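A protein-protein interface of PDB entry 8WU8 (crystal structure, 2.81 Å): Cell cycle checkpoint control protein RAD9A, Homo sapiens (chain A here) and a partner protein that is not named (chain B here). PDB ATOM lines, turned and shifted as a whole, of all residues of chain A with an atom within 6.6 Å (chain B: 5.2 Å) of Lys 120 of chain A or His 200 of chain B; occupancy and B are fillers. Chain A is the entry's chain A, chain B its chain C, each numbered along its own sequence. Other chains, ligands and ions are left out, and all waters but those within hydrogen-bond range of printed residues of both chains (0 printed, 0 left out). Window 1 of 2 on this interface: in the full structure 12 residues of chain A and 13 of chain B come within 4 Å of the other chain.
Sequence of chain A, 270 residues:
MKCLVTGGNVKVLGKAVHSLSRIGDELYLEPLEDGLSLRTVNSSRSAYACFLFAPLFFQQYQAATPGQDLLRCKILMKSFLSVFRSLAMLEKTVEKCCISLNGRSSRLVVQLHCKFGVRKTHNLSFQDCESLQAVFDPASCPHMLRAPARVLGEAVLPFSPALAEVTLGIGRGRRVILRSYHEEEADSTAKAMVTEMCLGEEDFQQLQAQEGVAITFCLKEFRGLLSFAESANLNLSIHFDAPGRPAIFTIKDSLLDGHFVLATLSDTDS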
ATOM      1  N   VAL A 110      10.136 -19.676 -25.338  1.00  0.00           N
ATOM      2  CA  VAL A 110       8.738 -20.054 -25.168  1.00  0.00           C
ATOM      3  C   VAL A 110       7.896 -19.373 -26.239  1.00  0.00           C
ATOM      4  O   VAL A 110       7.861 -18.147 -26.320  1.00  0.00           O
ATOM      5  CB  VAL A 110       8.198 -19.671 -23.774  1.00  0.00           C
ATOM      6  CG1 VAL A 110       6.703 -19.937 -23.696  1.00  0.00           C
ATOM      7  CG2 VAL A 110       8.937 -20.429 -22.682  1.00  0.00           C
ATOM      8  N   GLN A 111       7.228 -20.169 -27.066  1.00  0.00           N
ATOM      9  CA  GLN A 111       6.391 -19.623 -28.128  1.00  0.00           C
ATOM     10  C   GLN A 111       4.917 -19.867 -27.855  1.00  0.00           C
ATOM     11  O   GLN A 111       4.503 -20.996 -27.589  1.00  0.00           O
ATOM     12  CB  GLN A 111       6.772 -20.223 -29.486  1.00  0.00           C
ATOM     13  CG  GLN A 111       8.093 -19.724 -30.046  1.00  0.00           C
ATOM     14  CD  GLN A 111       8.319 -20.145 -31.488  1.00  0.00           C
ATOM     15  OE1 GLN A 111       7.528 -20.897 -32.060  1.00  0.00           O
ATOM     16  NE2 GLN A 111       9.401 -19.658 -32.084  1.00  0.00           N
ATOM     17  N   LEU A 112       4.129 -18.799 -27.926  1.00  0.00           N
ATOM     18  CA  LEU A 112       2.684 -18.897 -27.799  1.00  0.00           C
ATOM     19  C   LEU A 112       2.014 -18.728 -29.159  1.00  0.00           C
ATOM     20  O   LEU A 112       1.964 -17.621 -29.694  1.00  0.00           O
ATOM     21  CB  LEU A 112       2.155 -17.844 -26.824  1.00  0.00           C
ATOM     22  CG  LEU A 112       2.800 -17.782 -25.438  1.00  0.00           C
ATOM     23  CD1 LEU A 112       2.067 -16.785 -24.542  1.00  0.00           C
ATOM     24  CD2 LEU A 112       2.838 -19.161 -24.800  1.00  0.00           C
ATOM     25  N   HIS A 113       1.506 -19.824 -29.718  1.00  0.00           N
ATOM     26  CA  HIS A 113       0.788 -19.763 -30.990  1.00  0.00           C
ATOM     27  C   HIS A 113      -0.673 -19.395 -30.780  1.00  0.00           C
ATOM     28  O   HIS A 113      -1.504 -20.251 -30.483  1.00  0.00           O
ATOM     29  CB  HIS A 113       0.888 -21.093 -31.735  1.00  0.00           C
ATOM     30  CG  HIS A 113       2.245 -21.364 -32.300  1.00  0.00           C
ATOM     31  ND1 HIS A 113       3.272 -21.888 -31.545  1.00  0.00           N
ATOM     32  CD2 HIS A 113       2.750 -21.172 -33.541  1.00  0.00           C
ATOM     33  CE1 HIS A 113       4.350 -22.014 -32.300  1.00  0.00           C
ATOM     34  NE2 HIS A 113       4.058 -21.585 -33.516  1.00  0.00           N
ATOM     35  N   CYS A 114      -0.979 -18.114 -30.945  1.00  0.00           N
ATOM     36  CA  CYS A 114      -2.325 -17.613 -30.708  1.00  0.00           C
ATOM     37  C   CYS A 114      -3.176 -17.704 -31.967  1.00  0.00           C
ATOM     38  O   CYS A 114      -2.731 -18.224 -32.992  1.00  0.00           O
ATOM     39  CB  CYS A 114      -2.269 -16.169 -30.214  1.00  0.00           C
ATOM     40  SG  CYS A 114      -0.958 -15.865 -29.007  1.00  0.00           S
ATOM     41  N   VAL A 118      -1.256 -15.081 -35.074  1.00  0.00           N
ATOM     42  CA  VAL A 118      -0.464 -14.294 -34.135  1.00  0.00           C
ATOM     43  C   VAL A 118       0.417 -15.199 -33.284  1.00  0.00           C
ATOM     44  O   VAL A 118      -0.049 -16.195 -32.732  1.00  0.00           O
ATOM     45  CB  VAL A 118      -1.358 -13.439 -33.215  1.00  0.00           C
ATOM     46  CG1 VAL A 118      -0.513 -12.657 -32.222  1.00  0.00           C
ATOM     47  CG2 VAL A 118      -2.215 -12.494 -34.041  1.00  0.00           C
ATOM     48  N   ARG A 119       1.697 -14.851 -33.193  1.00  0.00           N
ATOM     49  CA  ARG A 119       2.654 -15.632 -32.422  1.00  0.00           C
ATOM     50  C   ARG A 119       3.371 -14.765 -31.397  1.00  0.00           C
ATOM     51  O   ARG A 119       3.909 -13.711 -31.731  1.00  0.00           O
ATOM     52  CB  ARG A 119       3.672 -16.300 -33.347  1.00  0.00           C
ATOM     53  CG  ARG A 119       4.834 -16.956 -32.619  1.00  0.00           C
ATOM     54  CD  ARG A 119       5.952 -17.331 -33.580  1.00  0.00           C
ATOM     55  NE  ARG A 119       5.507 -18.283 -34.593  1.00  0.00           N
ATOM     56  CZ  ARG A 119       6.290 -18.786 -35.543  1.00  0.00           C
ATOM     57  NH1 ARG A 119       7.565 -18.428 -35.612  1.00  0.00           N
ATOM     58  NH2 ARG A 119       5.797 -19.648 -36.423  1.00  0.00           N
ATOM     59  N   LYS A 120       3.363 -15.216 -30.146  1.00  0.00           N
ATOM     60  CA  LYS A 120       4.098 -14.553 -29.077  1.00  0.00           C
ATOM     61  C   LYS A 120       5.321 -15.390 -28.730  1.00  0.00           C
ATOM     62  O   LYS A 120       5.209 -16.600 -28.537  1.00  0.00           O
ATOM     63  CB  LYS A 120       3.211 -14.358 -27.847  1.00  0.00           C
ATOM     64  CG  LYS A 120       3.877 -13.634 -26.689  1.00  0.00           C
ATOM     65  CD  LYS A 120       3.993 -12.144 -26.956  1.00  0.00           C
ATOM     66  CE  LYS A 120       4.452 -11.399 -25.712  1.00  0.00           C
ATOM     67  NZ  LYS A 120       4.599  -9.937 -25.953  1.00  0.00           N
ATOM     68  N   THR A 121       6.486 -14.755 -28.656  1.00  0.00           N
ATOM     69  CA  THR A 121       7.727 -15.482 -28.404  1.00  0.00           C
ATOM     70  C   THR A 121       8.553 -14.869 -27.276  1.00  0.00           C
ATOM     71  O   THR A 121       8.903 -13.690 -27.320  1.00  0.00           O
ATOM     72  CB  THR A 121       8.598 -15.550 -29.671  1.00  0.00           C
ATOM     73  OG1 THR A 121       7.905 -16.277 -30.691  1.00  0.00           O
ATOM     74  CG2 THR A 121       9.915 -16.243 -29.377  1.00  0.00           C
ATOM     75  N   HIS A 122       8.864 -15.680 -26.269  1.00  0.00           N
ATOM     76  CA  HIS A 122       9.709 -15.245 -25.163  1.00  0.00           C
ATOM     77  C   HIS A 122      11.063 -15.942 -25.213  1.00  0.00           C
ATOM     78  O   HIS A 122      11.132 -17.158 -25.376  1.00  0.00           O
ATOM     79  CB  HIS A 122       9.033 -15.525 -23.818  1.00  0.00           C
ATOM     80  CG  HIS A 122       7.807 -14.705 -23.574  1.00  0.00           C
ATOM     81  ND1 HIS A 122       7.785 -13.644 -22.693  1.00  0.00           N
ATOM     82  CD2 HIS A 122       6.561 -14.786 -24.096  1.00  0.00           C
ATOM     83  CE1 HIS A 122       6.578 -13.108 -22.682  1.00  0.00           C
ATOM     84  NE2 HIS A 122       5.816 -13.782 -23.527  1.00  0.00           N
ATOM     85  N   ASN A 123      12.134 -15.167 -25.079  1.00  0.00           N
ATOM     86  CA  ASN A 123      13.476 -15.732 -24.982  1.00  0.00           C
ATOM     87  C   ASN A 123      14.066 -15.466 -23.606  1.00  0.00           C
ATOM     88  O   ASN A 123      14.808 -14.503 -23.412  1.00  0.00           O
ATOM     89  CB  ASN A 123      14.391 -15.164 -26.067  1.00  0.00           C
ATOM     90  CG  ASN A 123      14.056 -15.690 -27.447  1.00  0.00           C
ATOM     91  OD1 ASN A 123      13.426 -16.739 -27.588  1.00  0.00           O
ATOM     92  ND2 ASN A 123      14.483 -14.968 -28.476  1.00  0.00           N
ATOM     93  N   ARG B 189       6.180  -6.967 -36.388  1.00  0.00           N
ATOM     94  CA  ARG B 189       6.742  -7.498 -35.155  1.00  0.00           C
ATOM     95  C   ARG B 189       7.001  -6.406 -34.130  1.00  0.00           C
ATOM     96  O   ARG B 189       7.635  -5.395 -34.433  1.00  0.00           O
ATOM     97  CB  ARG B 189       8.042  -8.255 -35.443  1.00  0.00           C
ATOM     98  CG  ARG B 189       8.854  -8.591 -34.199  1.00  0.00           C
ATOM     99  CD  ARG B 189      10.125  -9.344 -34.548  1.00  0.00           C
ATOM    100  NE  ARG B 189       9.835 -10.674 -35.069  1.00  0.00           N
ATOM    101  CZ  ARG B 189      10.754 -11.504 -35.547  1.00  0.00           C
ATOM    102  NH1 ARG B 189      12.026 -11.138 -35.574  1.00  0.00           N
ATOM    103  NH2 ARG B 189      10.400 -12.698 -36.001  1.00  0.00           N
ATOM    104  N   LEU B 190       6.501  -6.618 -32.919  1.00  0.00           N
ATOM    105  CA  LEU B 190       6.783  -5.727 -31.803  1.00  0.00           C
ATOM    106  C   LEU B 190       7.767  -6.411 -30.868  1.00  0.00           C
ATOM    107  O   LEU B 190       7.590  -7.579 -30.526  1.00  0.00           O
ATOM    108  CB  LEU B 190       5.495  -5.352 -31.063  1.00  0.00           C
ATOM    109  CG  LEU B 190       4.827  -4.035 -31.463  1.00  0.00           C
ATOM    110  CD1 LEU B 190       4.703  -3.924 -32.969  1.00  0.00           C
ATOM    111  CD2 LEU B 190       3.459  -3.915 -30.808  1.00  0.00           C
ATOM    112  N   SER B 191       8.807  -5.690 -30.463  1.00  0.00           N
ATOM    113  CA  SER B 191       9.861  -6.285 -29.648  1.00  0.00           C
ATOM    114  C   SER B 191      10.243  -5.433 -28.438  1.00  0.00           C
ATOM    115  O   SER B 191      10.316  -4.205 -28.520  1.00  0.00           O
ATOM    116  CB  SER B 191      11.107  -6.540 -30.500  1.00  0.00           C
ATOM    117  OG  SER B 191      10.816  -7.388 -31.599  1.00  0.00           O
ATOM    118  N   THR B 192      10.479  -6.101 -27.312  1.00  0.00           N
ATOM    119  CA  THR B 192      11.036  -5.459 -26.130  1.00  0.00           C
ATOM    120  C   THR B 192      12.287  -6.218 -25.700  1.00  0.00           C
ATOM    121  O   THR B 192      12.410  -7.417 -25.949  1.00  0.00           O
ATOM    122  CB  THR B 192      10.036  -5.414 -24.964  1.00  0.00           C
ATOM    123  OG1 THR B 192       9.707  -6.747 -24.559  1.00  0.00           O
ATOM    124  CG2 THR B 192       8.768  -4.682 -25.376  1.00  0.00           C
ATOM    125  N   PHE B 193      13.216  -5.518 -25.060  1.00  0.00           N
ATOM    126  CA  PHE B 193      14.447  -6.140 -24.585  1.00  0.00           C
ATOM    127  C   PHE B 193      14.730  -5.726 -23.149  1.00  0.00           C
ATOM    128  O   PHE B 193      15.412  -4.733 -22.902  1.00  0.00           O
ATOM    129  CB  PHE B 193      15.623  -5.767 -25.490  1.00  0.00           C
ATOM    130  CG  PHE B 193      15.384  -6.058 -26.947  1.00  0.00           C
ATOM    131  CD1 PHE B 193      15.563  -7.335 -27.451  1.00  0.00           C
ATOM    132  CD2 PHE B 193      14.973  -5.053 -27.809  1.00  0.00           C
ATOM    133  CE1 PHE B 193      15.343  -7.606 -28.789  1.00  0.00           C
ATOM    134  CE2 PHE B 193      14.750  -5.319 -29.149  1.00  0.00           C
ATOM    135  CZ  PHE B 193      14.935  -6.599 -29.638  1.00  0.00           C
ATOM    136  N   SER B 198      13.839 -11.491 -23.788  1.00  0.00           N
ATOM    137  CA  SER B 198      13.602 -10.868 -25.081  1.00  0.00           C
ATOM    138  C   SER B 198      12.234 -11.309 -25.594  1.00  0.00           C
ATOM    139  O   SER B 198      12.016 -12.490 -25.863  1.00  0.00           O
ATOM    140  CB  SER B 198      14.704 -11.242 -26.073  1.00  0.00           C
ATOM    141  OG  SER B 198      14.460 -10.677 -27.344  1.00  0.00           O
ATOM    142  N   SER B 199      11.311 -10.361 -25.715  1.00  0.00           N
ATOM    143  CA  SER B 199       9.938 -10.677 -26.094  1.00  0.00           C
ATOM    144  C   SER B 199       9.577 -10.109 -27.464  1.00  0.00           C
ATOM    145  O   SER B 199       9.898  -8.961 -27.775  1.00  0.00           O
ATOM    146  CB  SER B 199       8.966 -10.150 -25.037  1.00  0.00           C
ATOM    147  OG  SER B 199       7.629 -10.503 -25.345  1.00  0.00           O
ATOM    148  N   HIS B 200       8.904 -10.922 -28.276  1.00  0.00           N
ATOM    149  CA  HIS B 200       8.491 -10.512 -29.616  1.00  0.00           C
ATOM    150  C   HIS B 200       7.023 -10.843 -29.869  1.00  0.00           C
ATOM    151  O   HIS B 200       6.436 -11.661 -29.164  1.00  0.00           O
ATOM    152  CB  HIS B 200       9.369 -11.183 -30.675  1.00  0.00           C
ATOM    153  CG  HIS B 200      10.837 -11.003 -30.444  1.00  0.00           C
ATOM    154  ND1 HIS B 200      11.483  -9.805 -30.662  1.00  0.00           N
ATOM    155  CD2 HIS B 200      11.784 -11.867 -30.012  1.00  0.00           C
ATOM    156  CE1 HIS B 200      12.765  -9.940 -30.374  1.00  0.00           C
ATOM    157  NE2 HIS B 200      12.975 -11.181 -29.977  1.00  0.00           N
ATOM    158  N   LEU B 201       6.431 -10.207 -30.876  1.00  0.00           N
ATOM    159  CA  LEU B 201       5.040 -10.481 -31.226  1.00  0.00           C
ATOM    160  C   LEU B 201       4.800 -10.328 -32.726  1.00  0.00           C
ATOM    161  O   LEU B 201       4.846  -9.221 -33.261  1.00  0.00           O
ATOM    162  CB  LEU B 201       4.103  -9.561 -30.447  1.00  0.00           C
ATOM    163  CG  LEU B 201       2.612  -9.847 -30.612  1.00  0.00           C
ATOM    164  CD1 LEU B 201       2.278 -11.248 -30.131  1.00  0.00           C
ATOM    165  CD2 LEU B 201       1.795  -8.821 -29.861  1.00  0.00           C
ATOM    166  N   ASP B 202       4.537 -11.447 -33.393  1.00  0.00           N
ATOM    167  CA  ASP B 202       4.384 -11.473 -34.845  1.00  0.00           C
ATOM    168  C   ASP B 202       2.937 -11.355 -35.300  1.00  0.00           C
ATOM    169  O   ASP B 202       2.045 -12.019 -34.773  1.00  0.00           O
ATOM    170  CB  ASP B 202       4.982 -12.758 -35.419  1.00  0.00           C
ATOM    171  CG  ASP B 202       6.492 -12.780 -35.347  1.00  0.00           C
ATOM    172  OD1 ASP B 202       7.063 -11.928 -34.632  1.00  0.00           O
ATOM    173  OD2 ASP B 202       7.108 -13.651 -36.000  1.00  0.00           O
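Of the 10 printed residues of chain B, 5 touch a printed residue of chain A. Of the 11 printed residues of chain A, 6 touch a printed residue of chain B. Among the printed residues, no Asp or Glu carboxylate lies within 4 Å of a Lys or Arg side-chain nitrogen of the other chain.
Lys 120 of chain A touches three residues of chain B. Printed residues of chain B within 4 Å of Thr 121 of chain A: Ser 198, Ser 199 and His 200. Of the printed residues of chain B, Asn 123 of chain A touches Ser 198 (2.8 Å). His 200 of chain B touches just these residues of chain A: Lys 120 (3.3 Å) and Thr 121 (2.9 Å). Of the printed residues of chain A, Leu 201 of chain B touches Val 118, Arg 119 and Lys 120.
O of Arg 119 of chain A is in hydrogen-bond range of N of Asp 202 of chain B, 2.9 Å away. The side-chain hydroxyl (OG) of Ser 199 of chain B sits at hydrogen-bond distance from the side-chain amino group (NZ) of Lys 120 of chain A (3.1 Å). O of Thr 121 of chain A lies within hydrogen-bond range of N of His 200 of chain B (2.9 Å). The backbone carbonyl oxygen (O) of Ser 198 of chain B lies within hydrogen-bond range of the backbone NH (N) of Asn 123 of chain A, 2.8 Å away.
Leu 201 of chain B touches Val 118 of chain A (CD1 to CG1, 3.8 Å). CA of Val 118 of chain A touches O of Asp 202 of chain B (3.4 Å). Leu 201 of chain B touches Arg 119 of chain A (CD1 to O, 3.4 Å). Lys 120 of chain A touches His 200 of chain B. Lys 120 of chain A touches Leu 201 of chain B (CD to CD1, 3.7 Å). Thr 121 of chain A touches Ser 198 of chain B (O to O, 3.6 Å). Ser 199 of chain B touches Thr 121 of chain A (CA to O, 3.4 Å). His 122 of chain A touches Ser 198 of chain B. His 122 of chain A touches Ser 199 of chain B.
The backbone carbonyl oxygen (O) of Ser 199 of chain B is in hydrogen-bond range of the backbone NH (N) of Thr 192 of chain B, at 3.0 Å. The backbone NH of His 122 of chain A sits at hydrogen-bond distance from the backbone carbonyl oxygen of Val 110 of chain A, 2.7 Å away. The side-chain hydroxyl (OG) of Ser 191 of chain B is in hydrogen-bond range of a ring nitrogen (ND1) of His 200 of chain B (2.7 Å). OG of Ser 198 of chain B sits at hydrogen-bond distance from NE2 of His 200 of chain B (3.1 Å). O of Leu 190 of chain B sits at hydrogen-bond distance from N of Leu 201 of chain B (2.9 Å). OD1 of Asp 202 of chain B is in salt-bridge range of NE of Arg 189 of chain B (3.1 Å).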
